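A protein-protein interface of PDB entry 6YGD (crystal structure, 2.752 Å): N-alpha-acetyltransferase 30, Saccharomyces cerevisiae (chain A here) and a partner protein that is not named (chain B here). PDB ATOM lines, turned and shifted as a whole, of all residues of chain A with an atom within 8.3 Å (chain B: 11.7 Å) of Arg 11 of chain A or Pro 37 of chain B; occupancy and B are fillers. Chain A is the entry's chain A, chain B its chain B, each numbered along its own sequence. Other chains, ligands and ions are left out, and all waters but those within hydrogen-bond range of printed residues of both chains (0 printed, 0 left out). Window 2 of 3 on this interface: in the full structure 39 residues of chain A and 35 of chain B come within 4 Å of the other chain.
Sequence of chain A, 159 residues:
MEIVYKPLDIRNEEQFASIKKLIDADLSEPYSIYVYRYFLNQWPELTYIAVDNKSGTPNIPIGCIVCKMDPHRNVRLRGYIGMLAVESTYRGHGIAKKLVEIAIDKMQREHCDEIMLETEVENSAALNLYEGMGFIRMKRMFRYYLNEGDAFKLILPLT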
ATOM      1  N   LEU A   8      39.113  13.843  -8.152  1.00  0.00           N
ATOM      2  CA  LEU A   8      37.853  14.559  -8.001  1.00  0.00           C
ATOM      3  C   LEU A   8      37.924  15.529  -6.829  1.00  0.00           C
ATOM      4  O   LEU A   8      38.472  15.210  -5.771  1.00  0.00           O
ATOM      5  CB  LEU A   8      36.703  13.574  -7.781  1.00  0.00           C
ATOM      6  CG  LEU A   8      35.434  14.173  -7.157  1.00  0.00           C
ATOM      7  CD1 LEU A   8      34.621  14.955  -8.187  1.00  0.00           C
ATOM      8  CD2 LEU A   8      34.589  13.111  -6.474  1.00  0.00           C
ATOM      9  N   ASP A   9      37.364  16.721  -7.022  1.00  0.00           N
ATOM     10  CA  ASP A   9      37.234  17.707  -5.959  1.00  0.00           C
ATOM     11  C   ASP A   9      35.810  17.640  -5.426  1.00  0.00           C
ATOM     12  O   ASP A   9      34.860  17.988  -6.134  1.00  0.00           O
ATOM     13  CB  ASP A   9      37.560  19.111  -6.464  1.00  0.00           C
ATOM     14  CG  ASP A   9      37.802  20.094  -5.336  1.00  0.00           C
ATOM     15  OD1 ASP A   9      37.607  19.716  -4.160  1.00  0.00           O
ATOM     16  OD2 ASP A   9      38.198  21.241  -5.626  1.00  0.00           O
ATOM     17  N   ILE A  10      35.668  17.197  -4.175  1.00  0.00           N
ATOM     18  CA  ILE A  10      34.345  16.897  -3.636  1.00  0.00           C
ATOM     19  C   ILE A  10      33.519  18.167  -3.439  1.00  0.00           C
ATOM     20  O   ILE A  10      32.285  18.129  -3.530  1.00  0.00           O
ATOM     21  CB  ILE A  10      34.489  16.077  -2.335  1.00  0.00           C
ATOM     22  CG1 ILE A  10      33.123  15.650  -1.796  1.00  0.00           C
ATOM     23  CG2 ILE A  10      35.283  16.843  -1.283  1.00  0.00           C
ATOM     24  CD1 ILE A  10      32.331  14.786  -2.748  1.00  0.00           C
ATOM     25  N   ARG A  11      34.169  19.309  -3.186  1.00  0.00           N
ATOM     26  CA  ARG A  11      33.419  20.538  -2.942  1.00  0.00           C
ATOM     27  C   ARG A  11      32.895  21.152  -4.235  1.00  0.00           C
ATOM     28  O   ARG A  11      31.887  21.869  -4.212  1.00  0.00           O
ATOM     29  CB  ARG A  11      34.278  21.562  -2.196  1.00  0.00           C
ATOM     30  CG  ARG A  11      34.872  21.072  -0.890  1.00  0.00           C
ATOM     31  CD  ARG A  11      36.343  20.743  -1.078  1.00  0.00           C
ATOM     32  NE  ARG A  11      37.133  21.937  -1.371  1.00  0.00           N
ATOM     33  CZ  ARG A  11      38.360  21.916  -1.882  1.00  0.00           C
ATOM     34  NH1 ARG A  11      38.939  20.757  -2.174  1.00  0.00           N
ATOM     35  NH2 ARG A  11      39.005  23.054  -2.108  1.00  0.00           N
ATOM     36  N   ASN A  12      33.560  20.893  -5.358  1.00  0.00           N
ATOM     37  CA  ASN A  12      33.157  21.478  -6.632  1.00  0.00           C
ATOM     38  C   ASN A  12      31.827  20.889  -7.090  1.00  0.00           C
ATOM     39  O   ASN A  12      31.702  19.671  -7.244  1.00  0.00           O
ATOM     40  CB  ASN A  12      34.238  21.236  -7.682  1.00  0.00           C
ATOM     41  CG  ASN A  12      33.926  21.903  -9.005  1.00  0.00           C
ATOM     42  OD1 ASN A  12      32.954  21.554  -9.671  1.00  0.00           O
ATOM     43  ND2 ASN A  12      34.774  22.841  -9.413  1.00  0.00           N
ATOM     44  N   GLU A  13      30.839  21.755  -7.327  1.00  0.00           N
ATOM     45  CA  GLU A  13      29.532  21.289  -7.788  1.00  0.00           C
ATOM     46  C   GLU A  13      29.565  20.905  -9.262  1.00  0.00           C
ATOM     47  O   GLU A  13      28.933  19.922  -9.667  1.00  0.00           O
ATOM     48  CB  GLU A  13      28.470  22.364  -7.541  1.00  0.00           C
ATOM     49  CG  GLU A  13      27.502  22.045  -6.403  1.00  0.00           C
ATOM     50  CD  GLU A  13      26.565  20.890  -6.730  1.00  0.00           C
ATOM     51  OE1 GLU A  13      25.850  20.973  -7.750  1.00  0.00           O
ATOM     52  OE2 GLU A  13      26.548  19.895  -5.974  1.00  0.00           O
ATOM     53  N   GLU A  14      30.295  21.673 -10.074  1.00  0.00           N
ATOM     54  CA  GLU A  14      30.306  21.453 -11.517  1.00  0.00           C
ATOM     55  C   GLU A  14      30.966  20.126 -11.876  1.00  0.00           C
ATOM     56  O   GLU A  14      30.489  19.415 -12.769  1.00  0.00           O
ATOM     57  CB  GLU A  14      31.014  22.616 -12.211  1.00  0.00           C
ATOM     58  CG  GLU A  14      30.252  23.931 -12.133  1.00  0.00           C
ATOM     59  CD  GLU A  14      31.169  25.128 -11.954  1.00  0.00           C
ATOM     60  OE1 GLU A  14      31.779  25.250 -10.869  1.00  0.00           O
ATOM     61  OE2 GLU A  14      31.285  25.941 -12.898  1.00  0.00           O
ATOM     62  N   GLN A  15      32.064  19.777 -11.201  1.00  0.00           N
ATOM     63  CA  GLN A  15      32.664  18.463 -11.410  1.00  0.00           C
ATOM     64  C   GLN A  15      31.649  17.363 -11.134  1.00  0.00           C
ATOM     65  O   GLN A  15      31.481  16.439 -11.938  1.00  0.00           O
ATOM     66  CB  GLN A  15      33.898  18.293 -10.523  1.00  0.00           C
ATOM     67  CG  GLN A  15      35.153  18.983 -11.040  1.00  0.00           C
ATOM     68  CD  GLN A  15      36.390  18.618 -10.238  1.00  0.00           C
ATOM     69  OE1 GLN A  15      36.319  17.857  -9.273  1.00  0.00           O
ATOM     70  NE2 GLN A  15      37.535  19.158 -10.639  1.00  0.00           N
ATOM     71  N   PHE A  16      30.945  17.464 -10.005  1.00  0.00           N
ATOM     72  CA  PHE A  16      29.923  16.480  -9.664  1.00  0.00           C
ATOM     73  C   PHE A  16      28.848  16.407 -10.744  1.00  0.00           C
ATOM     74  O   PHE A  16      28.492  15.319 -11.209  1.00  0.00           O
ATOM     75  CB  PHE A  16      29.308  16.829  -8.307  1.00  0.00           C
ATOM     76  CG  PHE A  16      28.615  15.679  -7.633  1.00  0.00           C
ATOM     77  CD1 PHE A  16      27.395  15.218  -8.097  1.00  0.00           C
ATOM     78  CD2 PHE A  16      29.173  15.076  -6.518  1.00  0.00           C
ATOM     79  CE1 PHE A  16      26.755  14.167  -7.474  1.00  0.00           C
ATOM     80  CE2 PHE A  16      28.534  14.025  -5.889  1.00  0.00           C
ATOM     81  CZ  PHE A  16      27.323  13.570  -6.369  1.00  0.00           C
ATOM     82  N   ARG A  37      26.443   9.648  -4.877  1.00  0.00           N
ATOM     83  CA  ARG A  37      26.717  10.115  -3.523  1.00  0.00           C
ATOM     84  C   ARG A  37      27.328   9.013  -2.668  1.00  0.00           C
ATOM     85  O   ARG A  37      28.165   9.292  -1.802  1.00  0.00           O
ATOM     86  CB  ARG A  37      25.432  10.644  -2.881  1.00  0.00           C
ATOM     87  CG  ARG A  37      25.634  11.876  -2.022  1.00  0.00           C
ATOM     88  CD  ARG A  37      25.921  13.105  -2.869  1.00  0.00           C
ATOM     89  NE  ARG A  37      26.557  14.159  -2.085  1.00  0.00           N
ATOM     90  CZ  ARG A  37      26.645  15.431  -2.460  1.00  0.00           C
ATOM     91  NH1 ARG A  37      26.125  15.825  -3.615  1.00  0.00           N
ATOM     92  NH2 ARG A  37      27.246  16.313  -1.674  1.00  0.00           N
ATOM     93  N   ASN A  41      31.200  10.536  -1.907  1.00  0.00           N
ATOM     94  CA  ASN A  41      31.347  11.074  -0.559  1.00  0.00           C
ATOM     95  C   ASN A  41      32.126  10.132   0.352  1.00  0.00           C
ATOM     96  O   ASN A  41      32.765  10.584   1.308  1.00  0.00           O
ATOM     97  CB  ASN A  41      29.975  11.382   0.046  1.00  0.00           C
ATOM     98  CG  ASN A  41      29.351  12.643  -0.527  1.00  0.00           C
ATOM     99  OD1 ASN A  41      29.288  12.825  -1.743  1.00  0.00           O
ATOM    100  ND2 ASN A  41      28.898  13.529   0.354  1.00  0.00           N
ATOM    101  N   PRO A  44      36.197   9.641  -1.969  1.00  0.00           N
ATOM    102  CA  PRO A  44      36.528  10.759  -2.868  1.00  0.00           C
ATOM    103  C   PRO A  44      37.897  10.628  -3.509  1.00  0.00           C
ATOM    104  O   PRO A  44      38.130  11.229  -4.566  1.00  0.00           O
ATOM    105  CB  PRO A  44      36.449  11.985  -1.947  1.00  0.00           C
ATOM    106  CG  PRO A  44      36.759  11.447  -0.593  1.00  0.00           C
ATOM    107  CD  PRO A  44      36.185  10.057  -0.554  1.00  0.00           C
ATOM    108  N   ASP B  29      16.850  25.009   3.415  1.00  0.00           N
ATOM    109  CA  ASP B  29      17.860  25.677   2.600  1.00  0.00           C
ATOM    110  C   ASP B  29      18.944  26.301   3.469  1.00  0.00           C
ATOM    111  O   ASP B  29      20.139  26.179   3.171  1.00  0.00           O
ATOM    112  CB  ASP B  29      17.199  26.738   1.719  1.00  0.00           C
ATOM    113  CG  ASP B  29      18.100  27.215   0.592  1.00  0.00           C
ATOM    114  OD1 ASP B  29      19.333  27.258   0.778  1.00  0.00           O
ATOM    115  OD2 ASP B  29      17.570  27.550  -0.488  1.00  0.00           O
ATOM    116  N   GLU B  30      18.546  26.963   4.556  1.00  0.00           N
ATOM    117  CA  GLU B  30      19.515  27.667   5.389  1.00  0.00           C
ATOM    118  C   GLU B  30      20.494  26.701   6.043  1.00  0.00           C
ATOM    119  O   GLU B  30      21.701  26.968   6.093  1.00  0.00           O
ATOM    120  CB  GLU B  30      18.788  28.495   6.447  1.00  0.00           C
ATOM    121  CG  GLU B  30      19.697  29.382   7.280  1.00  0.00           C
ATOM    122  CD  GLU B  30      20.288  30.531   6.485  1.00  0.00           C
ATOM    123  OE1 GLU B  30      19.842  30.769   5.342  1.00  0.00           O
ATOM    124  OE2 GLU B  30      21.202  31.202   7.007  1.00  0.00           O
ATOM    125  N   LEU B  31      19.997  25.571   6.544  1.00  0.00           N
ATOM    126  CA  LEU B  31      20.873  24.621   7.221  1.00  0.00           C
ATOM    127  C   LEU B  31      21.763  23.881   6.228  1.00  0.00           C
ATOM    128  O   LEU B  31      22.938  23.620   6.514  1.00  0.00           O
ATOM    129  CB  LEU B  31      20.037  23.641   8.048  1.00  0.00           C
ATOM    130  CG  LEU B  31      20.613  23.160   9.385  1.00  0.00           C
ATOM    131  CD1 LEU B  31      19.540  22.481  10.229  1.00  0.00           C
ATOM    132  CD2 LEU B  31      21.800  22.227   9.175  1.00  0.00           C
ATOM    133  N   CYS B  32      21.228  23.546   5.051  1.00  0.00           N
ATOM    134  CA  CYS B  32      22.002  22.785   4.072  1.00  0.00           C
ATOM    135  C   CYS B  32      23.104  23.630   3.447  1.00  0.00           C
ATOM    136  O   CYS B  32      24.168  23.106   3.096  1.00  0.00           O
ATOM    137  CB  CYS B  32      21.081  22.228   2.988  1.00  0.00           C
ATOM    138  SG  CYS B  32      19.938  20.963   3.569  1.00  0.00           S
ATOM    139  N   SER B  33      22.863  24.932   3.277  1.00  0.00           N
ATOM    140  CA  SER B  33      23.917  25.814   2.787  1.00  0.00           C
ATOM    141  C   SER B  33      25.082  25.858   3.765  1.00  0.00           C
ATOM    142  O   SER B  33      26.250  25.861   3.357  1.00  0.00           O
ATOM    143  CB  SER B  33      23.360  27.219   2.548  1.00  0.00           C
ATOM    144  OG  SER B  33      22.263  27.197   1.652  1.00  0.00           O
ATOM    145  N   LYS B  34      24.778  25.873   5.066  1.00  0.00           N
ATOM    146  CA  LYS B  34      25.811  25.917   6.096  1.00  0.00           C
ATOM    147  C   LYS B  34      26.678  24.665   6.088  1.00  0.00           C
ATOM    148  O   LYS B  34      27.884  24.741   6.351  1.00  0.00           O
ATOM    149  CB  LYS B  34      25.158  26.102   7.468  1.00  0.00           C
ATOM    150  CG  LYS B  34      25.957  25.556   8.642  1.00  0.00           C
ATOM    151  CD  LYS B  34      25.110  25.508   9.906  1.00  0.00           C
ATOM    152  CE  LYS B  34      25.854  24.835  11.049  1.00  0.00           C
ATOM    153  NZ  LYS B  34      24.990  24.717  12.258  1.00  0.00           N
ATOM    154  N   LEU B  35      26.092  23.516   5.773  1.00  0.00           N
ATOM    155  CA  LEU B  35      26.794  22.247   5.889  1.00  0.00           C
ATOM    156  C   LEU B  35      27.883  22.109   4.827  1.00  0.00           C
ATOM    157  O   LEU B  35      27.811  22.697   3.744  1.00  0.00           O
ATOM    158  CB  LEU B  35      25.798  21.096   5.779  1.00  0.00           C
ATOM    159  CG  LEU B  35      26.282  19.707   6.189  1.00  0.00           C
ATOM    160  CD1 LEU B  35      26.976  19.766   7.535  1.00  0.00           C
ATOM    161  CD2 LEU B  35      25.104  18.759   6.237  1.00  0.00           C
ATOM    162  N   LYS B  36      28.903  21.318   5.162  1.00  0.00           N
ATOM    163  CA  LYS B  36      30.020  21.080   4.261  1.00  0.00           C
ATOM    164  C   LYS B  36      29.555  20.326   3.016  1.00  0.00           C
ATOM    165  O   LYS B  36      28.637  19.505   3.087  1.00  0.00           O
ATOM    166  CB  LYS B  36      31.106  20.271   4.967  1.00  0.00           C
ATOM    167  CG  LYS B  36      31.461  20.763   6.356  1.00  0.00           C
ATOM    168  CD  LYS B  36      32.161  22.110   6.309  1.00  0.00           C
ATOM    169  CE  LYS B  36      32.538  22.577   7.708  1.00  0.00           C
ATOM    170  NZ  LYS B  36      33.281  23.867   7.700  1.00  0.00           N
ATOM    171  N   PRO B  37      30.187  20.579   1.862  1.00  0.00           N
ATOM    172  CA  PRO B  37      29.768  19.888   0.629  1.00  0.00           C
ATOM    173  C   PRO B  37      29.855  18.373   0.710  1.00  0.00           C
ATOM    174  O   PRO B  37      29.022  17.679   0.112  1.00  0.00           O
ATOM    175  CB  PRO B  37      30.727  20.454  -0.425  1.00  0.00           C
ATOM    176  CG  PRO B  37      31.148  21.775   0.117  1.00  0.00           C
ATOM    177  CD  PRO B  37      31.224  21.591   1.602  1.00  0.00           C
ATOM    178  N   GLU B  38      30.840  17.836   1.432  1.00  0.00           N
ATOM    179  CA  GLU B  38      31.038  16.393   1.487  1.00  0.00           C
ATOM    180  C   GLU B  38      30.175  15.711   2.539  1.00  0.00           C
ATOM    181  O   GLU B  38      30.001  14.488   2.475  1.00  0.00           O
ATOM    182  CB  GLU B  38      32.513  16.071   1.752  1.00  0.00           C
ATOM    183  CG  GLU B  38      33.075  16.632   3.059  1.00  0.00           C
ATOM    184  CD  GLU B  38      33.543  18.075   2.938  1.00  0.00           C
ATOM    185  OE1 GLU B  38      32.966  18.829   2.128  1.00  0.00           O
ATOM    186  OE2 GLU B  38      34.496  18.455   3.651  1.00  0.00           O
ATOM    187  N   ALA B  39      29.638  16.462   3.495  1.00  0.00           N
ATOM    188  CA  ALA B  39      28.901  15.856   4.595  1.00  0.00           C
ATOM    189  C   ALA B  39      27.514  15.419   4.143  1.00  0.00           C
ATOM    190  O   ALA B  39      26.888  16.060   3.295  1.00  0.00           O
ATOM    191  CB  ALA B  39      28.792  16.834   5.762  1.00  0.00           C
ATOM    192  N   ILE B  40      27.036  14.316   4.712  1.00  0.00           N
ATOM    193  CA  ILE B  40      25.706  13.789   4.425  1.00  0.00           C
ATOM    194  C   ILE B  40      24.990  13.553   5.744  1.00  0.00           C
ATOM    195  O   ILE B  40      25.523  12.877   6.630  1.00  0.00           O
ATOM    196  CB  ILE B  40      25.762  12.479   3.616  1.00  0.00           C
ATOM    197  CG1 ILE B  40      26.315  12.733   2.216  1.00  0.00           C
ATOM    198  CG2 ILE B  40      24.382  11.846   3.540  1.00  0.00           C
ATOM    199  CD1 ILE B  40      26.478  11.471   1.410  1.00  0.00           C
ATOM    200  N   VAL B  41      23.782  14.094   5.870  1.00  0.00           N
ATOM    201  CA  VAL B  41      22.984  13.911   7.076  1.00  0.00           C
ATOM    202  C   VAL B  41      22.149  12.651   6.907  1.00  0.00           C
ATOM    203  O   VAL B  41      21.269  12.588   6.047  1.00  0.00           O
ATOM    204  CB  VAL B  41      22.097  15.124   7.364  1.00  0.00           C
ATOM    205  CG1 VAL B  41      21.131  14.787   8.487  1.00  0.00           C
ATOM    206  CG2 VAL B  41      22.950  16.312   7.748  1.00  0.00           C
ATOM    207  N   LEU B  48      24.684   3.795   3.476  1.00  0.00           N
ATOM    208  CA  LEU B  48      24.477   4.552   2.246  1.00  0.00           C
ATOM    209  C   LEU B  48      24.346   3.657   1.022  1.00  0.00           C
ATOM    210  O   LEU B  48      23.909   4.133  -0.031  1.00  0.00           O
ATOM    211  CB  LEU B  48      25.621   5.541   2.035  1.00  0.00           C
ATOM    212  CG  LEU B  48      25.418   6.910   2.683  1.00  0.00           C
ATOM    213  CD1 LEU B  48      26.673   7.752   2.550  1.00  0.00           C
ATOM    214  CD2 LEU B  48      24.223   7.613   2.056  1.00  0.00           C
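Of the 12 printed residues of chain A, 4 touch a printed residue of chain B.
Printed residues of chain A that touch a printed residue of chain B: Ile 10, Arg 11, Arg 37 and Asn 41.
Of the 14 printed residues of chain B, 3 touch a printed residue of chain A.
Hydrophobic or aromatic side chains of chain B that line the printed part of chain A: Pro 37 and Ile 40.
Along chain B the printed residues that touch a printed residue of chain A span positions 37 to 40.
Among the printed residues, no Asp or Glu carboxylate lies within 4 Å of a Lys or Arg side-chain nitrogen of the other chain.
NH2 of Arg 37 of chain A lies within hydrogen-bond range of O of Pro 37 of chain B, 2.9 Å away.
ND2 of Asn 41 of chain A lies within hydrogen-bond range of O of Glu 38 of chain B.
Among the printed residues, pairs that only touch across the chains: Asn 41 of chain A with Ile 40 of chain B, Arg 37 of chain A with Ile 40 of chain B, Ile 10 of chain A with Glu 38 of chain B and Arg 11 of chain A with Pro 37 of chain B.
The guanidinium group (NH1) of Arg 11 of chain A lies within salt-bridge range of the side-chain carboxylate (OD1) of Asp 9 of chain A (2.6 Å).
The side-chain amide oxygen of Asn 41 of chain A is in hydrogen-bond range of the guanidinium group of Arg 37 of chain A (3.1 Å).
Of the printed residues of chain B, Arg 11 of chain A touches Pro 37.
Of chain A, only Arg 11 and Arg 37 come within 4 Å of Pro 37 of chain B.
No residue of chain B comes within 4 Å of Asp 9 of chain A.
Ile 10 of chain A touches one residue of chain B.
No residue of chain B comes within 4 Å of Asn 12 of chain A.
Of the printed residues of chain B, Asn 41 of chain A touches Glu 38 and Ile 40.
Of the printed residues of chain B, Arg 37 of chain A touches Pro 37 (2.9 Å) and Ile 40 (3.6 Å).
Printed residues of chain A within 4 Å of Ile 40 of chain B: Arg 37 (3.6 Å) and Asn 41 (3.3 Å).
The nearest printed residue of chain A that does not touch Pro 37 of chain B is Asn 41 of chain A (4.2 Å).
The nearest printed residue of chain A that does not touch Ile 40 of chain B is Ile 10 of chain A (7.9 Å).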
